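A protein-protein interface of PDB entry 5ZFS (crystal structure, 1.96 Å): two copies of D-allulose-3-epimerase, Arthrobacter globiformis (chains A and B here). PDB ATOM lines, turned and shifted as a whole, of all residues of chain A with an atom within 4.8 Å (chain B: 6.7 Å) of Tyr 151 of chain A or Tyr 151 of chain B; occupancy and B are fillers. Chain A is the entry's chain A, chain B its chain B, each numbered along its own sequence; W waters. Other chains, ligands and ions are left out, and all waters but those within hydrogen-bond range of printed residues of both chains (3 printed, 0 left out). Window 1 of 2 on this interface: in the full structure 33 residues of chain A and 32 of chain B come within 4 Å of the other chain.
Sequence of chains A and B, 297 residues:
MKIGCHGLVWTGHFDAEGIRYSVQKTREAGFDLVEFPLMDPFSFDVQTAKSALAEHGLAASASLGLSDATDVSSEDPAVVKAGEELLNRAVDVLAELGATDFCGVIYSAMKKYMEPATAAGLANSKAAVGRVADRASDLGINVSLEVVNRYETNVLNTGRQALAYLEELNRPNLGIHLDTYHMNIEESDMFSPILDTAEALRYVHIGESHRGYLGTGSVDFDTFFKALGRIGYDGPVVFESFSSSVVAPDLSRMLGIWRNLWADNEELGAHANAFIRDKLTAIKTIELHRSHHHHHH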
ATOM      1  N   LYS A 111      -5.606   7.365  -1.408  1.00  0.00           N
ATOM      2  CA  LYS A 111      -5.838   8.704  -0.877  1.00  0.00           C
ATOM      3  C   LYS A 111      -6.320   8.615   0.574  1.00  0.00           C
ATOM      4  O   LYS A 111      -6.744   7.553   1.031  1.00  0.00           O
ATOM      5  CB  LYS A 111      -6.889   9.430  -1.731  1.00  0.00           C
ATOM      6  CG  LYS A 111      -8.316   8.988  -1.443  1.00  0.00           C
ATOM      7  CD  LYS A 111      -9.338   9.678  -2.335  1.00  0.00           C
ATOM      8  CE  LYS A 111      -9.842  10.963  -1.717  1.00  0.00           C
ATOM      9  NZ  LYS A 111     -11.078  11.443  -2.383  1.00  0.00           N
ATOM     10  N   LYS A 112      -6.254   9.730   1.292  1.00  0.00           N
ATOM     11  CA  LYS A 112      -6.901   9.842   2.595  1.00  0.00           C
ATOM     12  C   LYS A 112      -8.350  10.282   2.409  1.00  0.00           C
ATOM     13  O   LYS A 112      -8.637  11.460   2.192  1.00  0.00           O
ATOM     14  CB  LYS A 112      -6.121  10.822   3.491  1.00  0.00           C
ATOM     15  CG  LYS A 112      -6.804  11.184   4.806  1.00  0.00           C
ATOM     16  CD  LYS A 112      -7.186   9.953   5.612  1.00  0.00           C
ATOM     17  CE  LYS A 112      -7.876  10.324   6.916  1.00  0.00           C
ATOM     18  NZ  LYS A 112      -8.938  11.355   6.738  1.00  0.00           N
ATOM     19  N   ASN A 149      -2.820   1.030   4.360  1.00  0.00           N
ATOM     20  CA  ASN A 149      -3.256   1.586   5.633  1.00  0.00           C
ATOM     21  C   ASN A 149      -4.412   2.577   5.491  1.00  0.00           C
ATOM     22  O   ASN A 149      -4.747   3.018   4.391  1.00  0.00           O
ATOM     23  CB  ASN A 149      -2.075   2.231   6.377  1.00  0.00           C
ATOM     24  CG  ASN A 149      -1.577   3.496   5.713  1.00  0.00           C
ATOM     25  OD1 ASN A 149      -2.299   4.480   5.618  1.00  0.00           O
ATOM     26  ND2 ASN A 149      -0.326   3.478   5.257  1.00  0.00           N
ATOM     27  N   ARG A 150      -5.007   2.921   6.631  1.00  0.00           N
ATOM     28  CA  ARG A 150      -6.219   3.730   6.698  1.00  0.00           C
ATOM     29  C   ARG A 150      -6.106   5.064   5.969  1.00  0.00           C
ATOM     30  O   ARG A 150      -7.123   5.658   5.593  1.00  0.00           O
ATOM     31  CB  ARG A 150      -6.566   3.995   8.169  1.00  0.00           C
ATOM     32  CG  ARG A 150      -5.511   4.824   8.899  1.00  0.00           C
ATOM     33  CD  ARG A 150      -5.708   4.777  10.407  1.00  0.00           C
ATOM     34  NE  ARG A 150      -5.739   3.398  10.893  1.00  0.00           N
ATOM     35  CZ  ARG A 150      -6.217   3.033  12.077  1.00  0.00           C
ATOM     36  NH1 ARG A 150      -6.681   3.948  12.918  1.00  0.00           N
ATOM     37  NH2 ARG A 150      -6.212   1.758  12.430  1.00  0.00           N
ATOM     38  N   TYR A 151      -4.886   5.565   5.793  1.00  0.00           N
ATOM     39  CA  TYR A 151      -4.710   6.872   5.174  1.00  0.00           C
ATOM     40  C   TYR A 151      -4.550   6.768   3.659  1.00  0.00           C
ATOM     41  O   TYR A 151      -4.379   7.782   2.991  1.00  0.00           O
ATOM     42  CB  TYR A 151      -3.488   7.617   5.725  1.00  0.00           C
ATOM     43  CG  TYR A 151      -3.404   7.766   7.225  1.00  0.00           C
ATOM     44  CD1 TYR A 151      -4.094   8.777   7.887  1.00  0.00           C
ATOM     45  CD2 TYR A 151      -2.590   6.934   7.973  1.00  0.00           C
ATOM     46  CE1 TYR A 151      -3.995   8.930   9.260  1.00  0.00           C
ATOM     47  CE2 TYR A 151      -2.479   7.082   9.341  1.00  0.00           C
ATOM     48  CZ  TYR A 151      -3.181   8.075   9.981  1.00  0.00           C
ATOM     49  OH  TYR A 151      -3.055   8.214  11.351  1.00  0.00           O
ATOM     50  N   GLU A 152      -4.591   5.551   3.125  1.00  0.00           N
ATOM     51  CA  GLU A 152      -4.416   5.346   1.691  1.00  0.00           C
ATOM     52  C   GLU A 152      -5.602   4.609   1.061  1.00  0.00           C
ATOM     53  O   GLU A 152      -5.751   4.605  -0.157  1.00  0.00           O
ATOM     54  CB  GLU A 152      -3.112   4.583   1.408  1.00  0.00           C
ATOM     55  CG  GLU A 152      -1.847   5.388   1.688  1.00  0.00           C
ATOM     56  CD  GLU A 152      -0.589   4.737   1.144  1.00  0.00           C
ATOM     57  OE1 GLU A 152      -0.683   3.933   0.185  1.00  0.00           O
ATOM     58  OE2 GLU A 152       0.505   5.020   1.684  1.00  0.00           O
ATOM     59  N   THR A 153      -6.445   3.991   1.888  1.00  0.00           N
ATOM     60  CA  THR A 153      -7.750   3.530   1.439  1.00  0.00           C
ATOM     61  C   THR A 153      -8.692   3.404   2.624  1.00  0.00           C
ATOM     62  O   THR A 153      -8.254   3.220   3.761  1.00  0.00           O
ATOM     63  CB  THR A 153      -7.677   2.167   0.723  1.00  0.00           C
ATOM     64  OG1 THR A 153      -8.980   1.814   0.225  1.00  0.00           O
ATOM     65  CG2 THR A 153      -7.211   1.074   1.677  1.00  0.00           C
ATOM     66  N   TYR A 181       5.145  -2.448   5.336  1.00  0.00           N
ATOM     67  CA  TYR A 181       4.964  -1.070   5.792  1.00  0.00           C
ATOM     68  C   TYR A 181       3.527  -0.830   6.249  1.00  0.00           C
ATOM     69  O   TYR A 181       3.292  -0.157   7.252  1.00  0.00           O
ATOM     70  CB  TYR A 181       5.319  -0.103   4.670  1.00  0.00           C
ATOM     71  CG  TYR A 181       4.796   1.300   4.865  1.00  0.00           C
ATOM     72  CD1 TYR A 181       5.440   2.194   5.710  1.00  0.00           C
ATOM     73  CD2 TYR A 181       3.665   1.737   4.187  1.00  0.00           C
ATOM     74  CE1 TYR A 181       4.965   3.481   5.883  1.00  0.00           C
ATOM     75  CE2 TYR A 181       3.183   3.024   4.352  1.00  0.00           C
ATOM     76  CZ  TYR A 181       3.837   3.892   5.203  1.00  0.00           C
ATOM     77  OH  TYR A 181       3.359   5.177   5.371  1.00  0.00           O
ATOM     78  N   HIS A 182       2.575  -1.378   5.504  1.00  0.00           N
ATOM     79  CA  HIS A 182       1.158  -1.220   5.826  1.00  0.00           C
ATOM     80  C   HIS A 182       0.707  -2.185   6.921  1.00  0.00           C
ATOM     81  O   HIS A 182      -0.140  -1.845   7.748  1.00  0.00           O
ATOM     82  CB  HIS A 182       0.304  -1.432   4.577  1.00  0.00           C
ATOM     83  CG  HIS A 182       0.494  -0.372   3.541  1.00  0.00           C
ATOM     84  ND1 HIS A 182       0.157   0.945   3.758  1.00  0.00           N
ATOM     85  CD2 HIS A 182       1.015  -0.428   2.292  1.00  0.00           C
ATOM     86  CE1 HIS A 182       0.456   1.656   2.684  1.00  0.00           C
ATOM     87  NE2 HIS A 182       0.968   0.844   1.777  1.00  0.00           N
ATOM     88  N   ARG A 211       9.609   3.720   5.392  1.00  0.00           N
ATOM     89  CA  ARG A 211       9.862   3.524   3.961  1.00  0.00           C
ATOM     90  C   ARG A 211      11.257   3.963   3.518  1.00  0.00           C
ATOM     91  O   ARG A 211      11.483   4.232   2.337  1.00  0.00           O
ATOM     92  CB  ARG A 211       8.795   4.214   3.109  1.00  0.00           C
ATOM     93  CG  ARG A 211       7.373   3.949   3.574  1.00  0.00           C
ATOM     94  CD  ARG A 211       6.360   4.326   2.509  1.00  0.00           C
ATOM     95  NE  ARG A 211       5.852   3.158   1.799  1.00  0.00           N
ATOM     96  CZ  ARG A 211       4.687   3.134   1.167  1.00  0.00           C
ATOM     97  NH1 ARG A 211       3.925   4.220   1.149  1.00  0.00           N
ATOM     98  NH2 ARG A 211       4.285   2.029   0.555  1.00  0.00           N
ATOM     99  N   LEU A 255       1.753   9.764  -1.418  1.00  0.00           N
ATOM    100  CA  LEU A 255       2.227   8.907  -0.338  1.00  0.00           C
ATOM    101  C   LEU A 255       2.841   9.721   0.793  1.00  0.00           C
ATOM    102  O   LEU A 255       3.311   9.160   1.784  1.00  0.00           O
ATOM    103  CB  LEU A 255       3.244   7.892  -0.863  1.00  0.00           C
ATOM    104  CG  LEU A 255       2.705   6.890  -1.889  1.00  0.00           C
ATOM    105  CD1 LEU A 255       3.780   5.889  -2.281  1.00  0.00           C
ATOM    106  CD2 LEU A 255       1.489   6.168  -1.335  1.00  0.00           C
ATOM    107  N   MET B 110      -4.243  19.089  11.076  1.00  0.00           N
ATOM    108  CA  MET B 110      -4.131  17.653  11.277  1.00  0.00           C
ATOM    109  C   MET B 110      -4.807  16.960  10.101  1.00  0.00           C
ATOM    110  O   MET B 110      -6.023  16.754  10.101  1.00  0.00           O
ATOM    111  CB  MET B 110      -4.803  17.256  12.595  1.00  0.00           C
ATOM    112  CG  MET B 110      -4.626  15.801  13.006  1.00  0.00           C
ATOM    113  SD  MET B 110      -5.279  15.488  14.666  1.00  0.00           S
ATOM    114  CE  MET B 110      -7.032  15.667  14.385  1.00  0.00           C
ATOM    115  N   LYS B 111      -4.012  16.629   9.093  1.00  0.00           N
ATOM    116  CA  LYS B 111      -4.542  16.317   7.772  1.00  0.00           C
ATOM    117  C   LYS B 111      -3.451  15.717   6.896  1.00  0.00           C
ATOM    118  O   LYS B 111      -2.263  15.824   7.203  1.00  0.00           O
ATOM    119  CB  LYS B 111      -5.108  17.574   7.097  1.00  0.00           C
ATOM    120  CG  LYS B 111      -4.053  18.469   6.459  1.00  0.00           C
ATOM    121  CD  LYS B 111      -4.668  19.656   5.722  1.00  0.00           C
ATOM    122  CE  LYS B 111      -4.373  19.591   4.239  1.00  0.00           C
ATOM    123  NZ  LYS B 111      -5.060  20.661   3.466  1.00  0.00           N
ATOM    124  N   LYS B 112      -3.874  15.080   5.808  1.00  0.00           N
ATOM    125  CA  LYS B 112      -2.961  14.627   4.768  1.00  0.00           C
ATOM    126  C   LYS B 112      -2.697  15.767   3.793  1.00  0.00           C
ATOM    127  O   LYS B 112      -3.520  16.041   2.924  1.00  0.00           O
ATOM    128  CB  LYS B 112      -3.569  13.425   4.037  1.00  0.00           C
ATOM    129  CG  LYS B 112      -2.810  12.973   2.794  1.00  0.00           C
ATOM    130  CD  LYS B 112      -1.324  12.793   3.051  1.00  0.00           C
ATOM    131  CE  LYS B 112      -0.597  12.224   1.835  1.00  0.00           C
ATOM    132  NZ  LYS B 112      -0.938  12.928   0.564  1.00  0.00           N
ATOM    133  N   TYR B 113      -1.556  16.437   3.942  1.00  0.00           N
ATOM    134  CA  TYR B 113      -1.158  17.479   3.005  1.00  0.00           C
ATOM    135  C   TYR B 113      -0.822  16.876   1.649  1.00  0.00           C
ATOM    136  O   TYR B 113      -0.476  15.699   1.554  1.00  0.00           O
ATOM    137  CB  TYR B 113       0.052  18.264   3.536  1.00  0.00           C
ATOM    138  CG  TYR B 113      -0.275  19.238   4.654  1.00  0.00           C
ATOM    139  CD1 TYR B 113      -0.240  18.839   5.979  1.00  0.00           C
ATOM    140  CD2 TYR B 113      -0.618  20.559   4.379  1.00  0.00           C
ATOM    141  CE1 TYR B 113      -0.529  19.724   7.007  1.00  0.00           C
ATOM    142  CE2 TYR B 113      -0.921  21.450   5.398  1.00  0.00           C
ATOM    143  CZ  TYR B 113      -0.867  21.033   6.711  1.00  0.00           C
ATOM    144  OH  TYR B 113      -1.159  21.912   7.741  1.00  0.00           O
ATOM    145  N   VAL B 148       3.452  13.667  14.883  1.00  0.00           N
ATOM    146  CA  VAL B 148       2.527  12.717  14.278  1.00  0.00           C
ATOM    147  C   VAL B 148       3.021  12.331  12.891  1.00  0.00           C
ATOM    148  O   VAL B 148       3.930  12.958  12.344  1.00  0.00           O
ATOM    149  CB  VAL B 148       1.093  13.278  14.184  1.00  0.00           C
ATOM    150  CG1 VAL B 148       0.562  13.643  15.561  1.00  0.00           C
ATOM    151  CG2 VAL B 148       1.036  14.474  13.243  1.00  0.00           C
ATOM    152  N   ASN B 149       2.412  11.299  12.322  1.00  0.00           N
ATOM    153  CA  ASN B 149       2.941  10.684  11.120  1.00  0.00           C
ATOM    154  C   ASN B 149       2.640  11.516   9.863  1.00  0.00           C
ATOM    155  O   ASN B 149       1.879  12.488   9.906  1.00  0.00           O
ATOM    156  CB  ASN B 149       2.403   9.262  10.985  1.00  0.00           C
ATOM    157  CG  ASN B 149       0.923   9.226  10.673  1.00  0.00           C
ATOM    158  OD1 ASN B 149       0.488   9.709   9.629  1.00  0.00           O
ATOM    159  ND2 ASN B 149       0.136   8.667  11.585  1.00  0.00           N
ATOM    160  N   ARG B 150       3.263  11.117   8.756  1.00  0.00           N
ATOM    161  CA  ARG B 150       3.277  11.880   7.505  1.00  0.00           C
ATOM    162  C   ARG B 150       1.872  12.170   6.967  1.00  0.00           C
ATOM    163  O   ARG B 150       1.682  13.097   6.172  1.00  0.00           O
ATOM    164  CB  ARG B 150       4.061  11.092   6.454  1.00  0.00           C
ATOM    165  CG  ARG B 150       3.402   9.772   6.069  1.00  0.00           C
ATOM    166  CD  ARG B 150       4.373   8.805   5.385  1.00  0.00           C
ATOM    167  NE  ARG B 150       5.625   8.668   6.121  1.00  0.00           N
ATOM    168  CZ  ARG B 150       6.753   8.179   5.607  1.00  0.00           C
ATOM    169  NH1 ARG B 150       6.793   7.746   4.352  1.00  0.00           N
ATOM    170  NH2 ARG B 150       7.845   8.109   6.355  1.00  0.00           N
ATOM    171  N   TYR B 151       0.898  11.368   7.383  1.00  0.00           N
ATOM    172  CA  TYR B 151      -0.472  11.505   6.884  1.00  0.00           C
ATOM    173  C   TYR B 151      -1.318  12.455   7.737  1.00  0.00           C
ATOM    174  O   TYR B 151      -2.492  12.705   7.425  1.00  0.00           O
ATOM    175  CB  TYR B 151      -1.168  10.156   6.849  1.00  0.00           C
ATOM    176  CG  TYR B 151      -0.487   9.078   6.032  1.00  0.00           C
ATOM    177  CD1 TYR B 151      -0.539   9.085   4.643  1.00  0.00           C
ATOM    178  CD2 TYR B 151       0.161   8.020   6.657  1.00  0.00           C
ATOM    179  CE1 TYR B 151       0.054   8.078   3.899  1.00  0.00           C
ATOM    180  CE2 TYR B 151       0.755   7.009   5.924  1.00  0.00           C
ATOM    181  CZ  TYR B 151       0.705   7.042   4.552  1.00  0.00           C
ATOM    182  OH  TYR B 151       1.294   6.029   3.836  1.00  0.00           O
ATOM    183  N   GLU B 152      -0.736  12.967   8.816  1.00  0.00           N
ATOM    184  CA  GLU B 152      -1.452  13.850   9.736  1.00  0.00           C
ATOM    185  C   GLU B 152      -0.753  15.206   9.870  1.00  0.00           C
ATOM    186  O   GLU B 152      -1.351  16.175  10.328  1.00  0.00           O
ATOM    187  CB  GLU B 152      -1.610  13.189  11.111  1.00  0.00           C
ATOM    188  CG  GLU B 152      -2.678  12.104  11.143  1.00  0.00           C
ATOM    189  CD  GLU B 152      -2.978  11.600  12.542  1.00  0.00           C
ATOM    190  OE1 GLU B 152      -2.838  12.382  13.513  1.00  0.00           O
ATOM    191  OE2 GLU B 152      -3.354  10.416  12.673  1.00  0.00           O
ATOM    192  N   THR B 153       0.505  15.283   9.442  1.00  0.00           N
ATOM    193  CA  THR B 153       1.161  16.574   9.270  1.00  0.00           C
ATOM    194  C   THR B 153       2.339  16.442   8.315  1.00  0.00           C
ATOM    195  O   THR B 153       2.869  15.341   8.118  1.00  0.00           O
ATOM    196  CB  THR B 153       1.654  17.155  10.610  1.00  0.00           C
ATOM    197  OG1 THR B 153       2.164  18.480  10.405  1.00  0.00           O
ATOM    198  CG2 THR B 153       2.745  16.284  11.218  1.00  0.00           C
ATOM    199  N   ASN B 154       2.736  17.565   7.722  1.00  0.00           N
ATOM    200  CA  ASN B 154       3.997  17.637   6.990  1.00  0.00           C
ATOM    201  C   ASN B 154       5.067  18.444   7.718  1.00  0.00           C
ATOM    202  O   ASN B 154       6.132  18.730   7.165  1.00  0.00           O
ATOM    203  CB  ASN B 154       3.774  18.192   5.581  1.00  0.00           C
ATOM    204  CG  ASN B 154       3.187  19.592   5.582  1.00  0.00           C
ATOM    205  OD1 ASN B 154       2.905  20.165   6.640  1.00  0.00           O
ATOM    206  ND2 ASN B 154       3.000  20.158   4.386  1.00  0.00           N
ATOM    207  N   ASN B 157       7.167  15.311  11.995  1.00  0.00           N
ATOM    208  CA  ASN B 157       6.955  13.868  11.882  1.00  0.00           C
ATOM    209  C   ASN B 157       7.890  13.055  12.790  1.00  0.00           C
ATOM    210  O   ASN B 157       7.647  11.872  13.021  1.00  0.00           O
ATOM    211  CB  ASN B 157       7.173  13.393  10.435  1.00  0.00           C
ATOM    212  CG  ASN B 157       6.172  13.979   9.457  1.00  0.00           C
ATOM    213  OD1 ASN B 157       6.543  14.397   8.360  1.00  0.00           O
ATOM    214  ND2 ASN B 157       4.906  14.001   9.836  1.00  0.00           N
ATOM    215  N   TYR B 181       1.839   5.277  18.716  1.00  0.00           N
ATOM    216  CA  TYR B 181       1.236   4.940  17.419  1.00  0.00           C
ATOM    217  C   TYR B 181       1.973   5.645  16.280  1.00  0.00           C
ATOM    218  O   TYR B 181       2.227   5.057  15.229  1.00  0.00           O
ATOM    219  CB  TYR B 181      -0.237   5.337  17.430  1.00  0.00           C
ATOM    220  CG  TYR B 181      -0.902   5.458  16.080  1.00  0.00           C
ATOM    221  CD1 TYR B 181      -1.365   4.331  15.405  1.00  0.00           C
ATOM    222  CD2 TYR B 181      -1.107   6.703  15.500  1.00  0.00           C
ATOM    223  CE1 TYR B 181      -1.992   4.442  14.178  1.00  0.00           C
ATOM    224  CE2 TYR B 181      -1.733   6.824  14.272  1.00  0.00           C
ATOM    225  CZ  TYR B 181      -2.171   5.692  13.614  1.00  0.00           C
ATOM    226  OH  TYR B 181      -2.804   5.809  12.396  1.00  0.00           O
ATOM    227  N   HIS B 182       2.328   6.905  16.495  1.00  0.00           N
ATOM    228  CA  HIS B 182       3.041   7.672  15.477  1.00  0.00           C
ATOM    229  C   HIS B 182       4.519   7.303  15.417  1.00  0.00           C
ATOM    230  O   HIS B 182       5.101   7.200  14.329  1.00  0.00           O
ATOM    231  CB  HIS B 182       2.865   9.170  15.719  1.00  0.00           C
ATOM    232  CG  HIS B 182       1.451   9.637  15.577  1.00  0.00           C
ATOM    233  ND1 HIS B 182       0.769   9.585  14.379  1.00  0.00           N
ATOM    234  CD2 HIS B 182       0.586  10.155  16.480  1.00  0.00           C
ATOM    235  CE1 HIS B 182      -0.452  10.059  14.551  1.00  0.00           C
ATOM    236  NE2 HIS B 182      -0.589  10.409  15.815  1.00  0.00           N
ATOM    237  N   ILE B 185       5.521   4.413  13.247  1.00  0.00           N
ATOM    238  CA  ILE B 185       5.668   4.655  11.824  1.00  0.00           C
ATOM    239  C   ILE B 185       6.998   5.344  11.505  1.00  0.00           C
ATOM    240  O   ILE B 185       7.811   4.796  10.761  1.00  0.00           O
ATOM    241  CB  ILE B 185       4.477   5.454  11.257  1.00  0.00           C
ATOM    242  CG1 ILE B 185       3.185   4.648  11.412  1.00  0.00           C
ATOM    243  CG2 ILE B 185       4.692   5.765   9.785  1.00  0.00           C
ATOM    244  CD1 ILE B 185       1.941   5.506  11.415  1.00  0.00           C
ATOM    245  N   GLU B 186       7.226   6.522  12.071  1.00  0.00           N
ATOM    246  CA  GLU B 186       8.224   7.454  11.527  1.00  0.00           C
ATOM    247  C   GLU B 186       9.615   7.311  12.144  1.00  0.00           C
ATOM    248  O   GLU B 186      10.613   7.715  11.532  1.00  0.00           O
ATOM    249  CB  GLU B 186       7.770   8.901  11.685  1.00  0.00           C
ATOM    250  CG  GLU B 186       6.434   9.224  11.032  1.00  0.00           C
ATOM    251  CD  GLU B 186       6.489   9.235   9.517  1.00  0.00           C
ATOM    252  OE1 GLU B 186       7.612   9.243   8.937  1.00  0.00           O
ATOM    253  OE2 GLU B 186       5.400   9.244   8.898  1.00  0.00           O
ATOM    254  N   ARG B 211      -4.410   1.455  16.841  1.00  0.00           N
ATOM    255  CA  ARG B 211      -5.174   2.285  17.771  1.00  0.00           C
ATOM    256  C   ARG B 211      -6.332   1.533  18.438  1.00  0.00           C
ATOM    257  O   ARG B 211      -7.283   2.155  18.924  1.00  0.00           O
ATOM    258  CB  ARG B 211      -5.685   3.558  17.085  1.00  0.00           C
ATOM    259  CG  ARG B 211      -4.603   4.342  16.358  1.00  0.00           C
ATOM    260  CD  ARG B 211      -5.029   5.767  16.037  1.00  0.00           C
ATOM    261  NE  ARG B 211      -4.375   6.746  16.901  1.00  0.00           N
ATOM    262  CZ  ARG B 211      -4.124   7.999  16.544  1.00  0.00           C
ATOM    263  NH1 ARG B 211      -4.471   8.429  15.337  1.00  0.00           N
ATOM    264  NH2 ARG B 211      -3.531   8.823  17.391  1.00  0.00           N
ATOM    265  N   MET B 254     -11.033  12.604  10.405  1.00  0.00           N
ATOM    266  CA  MET B 254      -9.708  13.168  10.175  1.00  0.00           C
ATOM    267  C   MET B 254      -8.626  12.106  10.402  1.00  0.00           C
ATOM    268  O   MET B 254      -7.613  12.072   9.691  1.00  0.00           O
ATOM    269  CB  MET B 254      -9.485  14.380  11.087  1.00  0.00           C
ATOM    270  CG  MET B 254     -10.342  15.585  10.713  1.00  0.00           C
ATOM    271  SD  MET B 254     -10.402  16.855  11.999  1.00  0.00           S
ATOM    272  CE  MET B 254      -8.972  17.852  11.592  1.00  0.00           C
ATOM    273  N   LEU B 255      -8.859  11.233  11.380  1.00  0.00           N
ATOM    274  CA  LEU B 255      -7.901  10.204  11.755  1.00  0.00           C
ATOM    275  C   LEU B 255      -8.072   8.892  10.987  1.00  0.00           C
ATOM    276  O   LEU B 255      -7.312   7.944  11.197  1.00  0.00           O
ATOM    277  CB  LEU B 255      -7.998   9.924  13.255  1.00  0.00           C
ATOM    278  CG  LEU B 255      -7.724  11.115  14.179  1.00  0.00           C
ATOM    279  CD1 LEU B 255      -7.882  10.690  15.630  1.00  0.00           C
ATOM    280  CD2 LEU B 255      -6.330  11.671  13.930  1.00  0.00           C
ATOM    281  N   GLY B 256      -9.060   8.833  10.099  1.00  0.00           N
ATOM    282  CA  GLY B 256      -9.263   7.655   9.258  1.00  0.00           C
ATOM    283  C   GLY B 256      -9.693   6.420  10.032  1.00  0.00           C
ATOM    284  O   GLY B 256      -9.206   5.316   9.789  1.00  0.00           O
ATOM    285  N   TRP B 258     -11.785   3.761  10.246  1.00  0.00           N
ATOM    286  CA  TRP B 258     -12.755   3.063   9.412  1.00  0.00           C
ATOM    287  C   TRP B 258     -13.249   1.780  10.065  1.00  0.00           C
ATOM    288  O   TRP B 258     -14.300   1.242   9.689  1.00  0.00           O
ATOM    289  CB  TRP B 258     -12.166   2.734   8.037  1.00  0.00           C
ATOM    290  CG  TRP B 258     -11.413   3.863   7.375  1.00  0.00           C
ATOM    291  CD1 TRP B 258     -10.170   3.792   6.830  1.00  0.00           C
ATOM    292  CD2 TRP B 258     -11.861   5.214   7.176  1.00  0.00           C
ATOM    293  NE1 TRP B 258      -9.808   5.008   6.307  1.00  0.00           N
ATOM    294  CE2 TRP B 258     -10.826   5.900   6.508  1.00  0.00           C
ATOM    295  CE3 TRP B 258     -13.030   5.908   7.501  1.00  0.00           C
ATOM    296  CZ2 TRP B 258     -10.923   7.246   6.157  1.00  0.00           C
ATOM    297  CZ3 TRP B 258     -13.127   7.245   7.156  1.00  0.00           C
ATOM    298  CH2 TRP B 258     -12.077   7.902   6.489  1.00  0.00           C
HETATM  299  O   HOH W   1       4.163   6.791   2.659  1.00  0.00           O
HETATM  300  O   HOH W   2      -5.610   6.937  12.932  1.00  0.00           O
HETATM  301  O   HOH W   3      -7.525  13.756   6.951  1.00  0.00           O
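Water W1 lies within hydrogen-bond range of O of Leu 255 of chain A (2.7 Å), NH1 of Arg 211 of chain A (3.0 Å), OH of Tyr 151 of chain B (3.2 Å), OH of Tyr 181 of chain A (3.3 Å) and NH1 of Arg 150 of chain B (3.3 Å).
Water W3 bridges NZ of Lys 112 of chain A (2.8 Å) and O of Met 254 of chain B (3.2 Å).
Of the 11 printed residues of chain A, 9 touch a printed residue of chain B.
Along chain A the printed residues that touch a printed residue of chain B span positions 112 to 255.
Of the 21 printed residues of chain B, 11 touch a printed residue of chain A.
Hydrophobic or aromatic side chains of chain B that line the printed part of chain A: Tyr 151, Tyr 181 and Trp 258.
Among the printed residues, 20 pairs touch across the chains.
Among the printed residues, no Asp or Glu carboxylate lies within 4 Å of a Lys or Arg side-chain nitrogen of the other chain.
Tyr 151 of chain A touches Tyr 181 of chain B, and with the chains exchanged Tyr 181 of chain A touches Tyr 151 of chain B.
Tyr 151 of chain A touches Leu 255 of chain B, but with the chains exchanged Leu 255 of chain A does not touch Tyr 151 of chain B (4.03 Å).
Lys 112 of chain A touches Lys 112 of chain B.
CE of Lys 112 of chain A touches N of Gly 256 of chain B, at 3.7 Å.
Arg 150 of chain A touches Tyr 181 of chain B (CD to OH, 3.7 Å).
Arg 150 of chain A touches Leu 255 of chain B (CD to O, 3.6 Å).
Tyr 151 of chain B touches Tyr 151 of chain A (CD2 to CD2, 3.2 Å).
O of Met 254 of chain B sits close to NZ of Lys 112 of chain A, at 3.3 Å.
ND2 of Asn 149 of chain A sits at hydrogen-bond distance from OH of Tyr 151 of chain B, at 3.3 Å.
The backbone carbonyl oxygen (O) of Arg 150 of chain A is in hydrogen-bond range of the indole nitrogen (NE1) of Trp 258 of chain B, at 2.9 Å.
ND2 of Asn 149 of chain B sits at hydrogen-bond distance from OH of Tyr 151 of chain A (3.2 Å).
The side-chain hydroxyl (OH) of Tyr 151 of chain A is in hydrogen-bond range of the side-chain carboxylate (OE2) of Glu 152 of chain B, at 2.6 Å.
The side-chain hydroxyl (OH) of Tyr 181 of chain B sits at hydrogen-bond distance from the side-chain hydroxyl (OH) of Tyr 151 of chain A (2.6 Å).
OH of Tyr 151 of chain B lies within hydrogen-bond range of OE2 of Glu 152 of chain A, 2.5 Å away.
NE1 of Trp 258 of chain B lies within hydrogen-bond range of O of Thr 153 of chain A.
OH of Tyr 181 of chain A is in hydrogen-bond range of OH of Tyr 151 of chain B (2.7 Å).
The backbone NH (N) of Lys 111 of chain B lies within hydrogen-bond range of the backbone carbonyl oxygen (O) of Glu 152 of chain B, 3.0 Å away.
The backbone NH (N) of Arg 150 of chain B lies close to the side-chain amide nitrogen (ND2) of Asn 157 of chain B, 3.5 Å away.
Tyr 151 of chain A touches five residues of chain B.
Tyr 151 of chain B touches four residues of chain A.
Of the printed residues of chain B, Glu 152 of chain A touches Tyr 151 (2.5 Å).
Of the printed residues of chain A, Gly 256 of chain B touches Lys 112 and Arg 150.
Thr 153 of chain B touches none of the printed residues of chain A.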
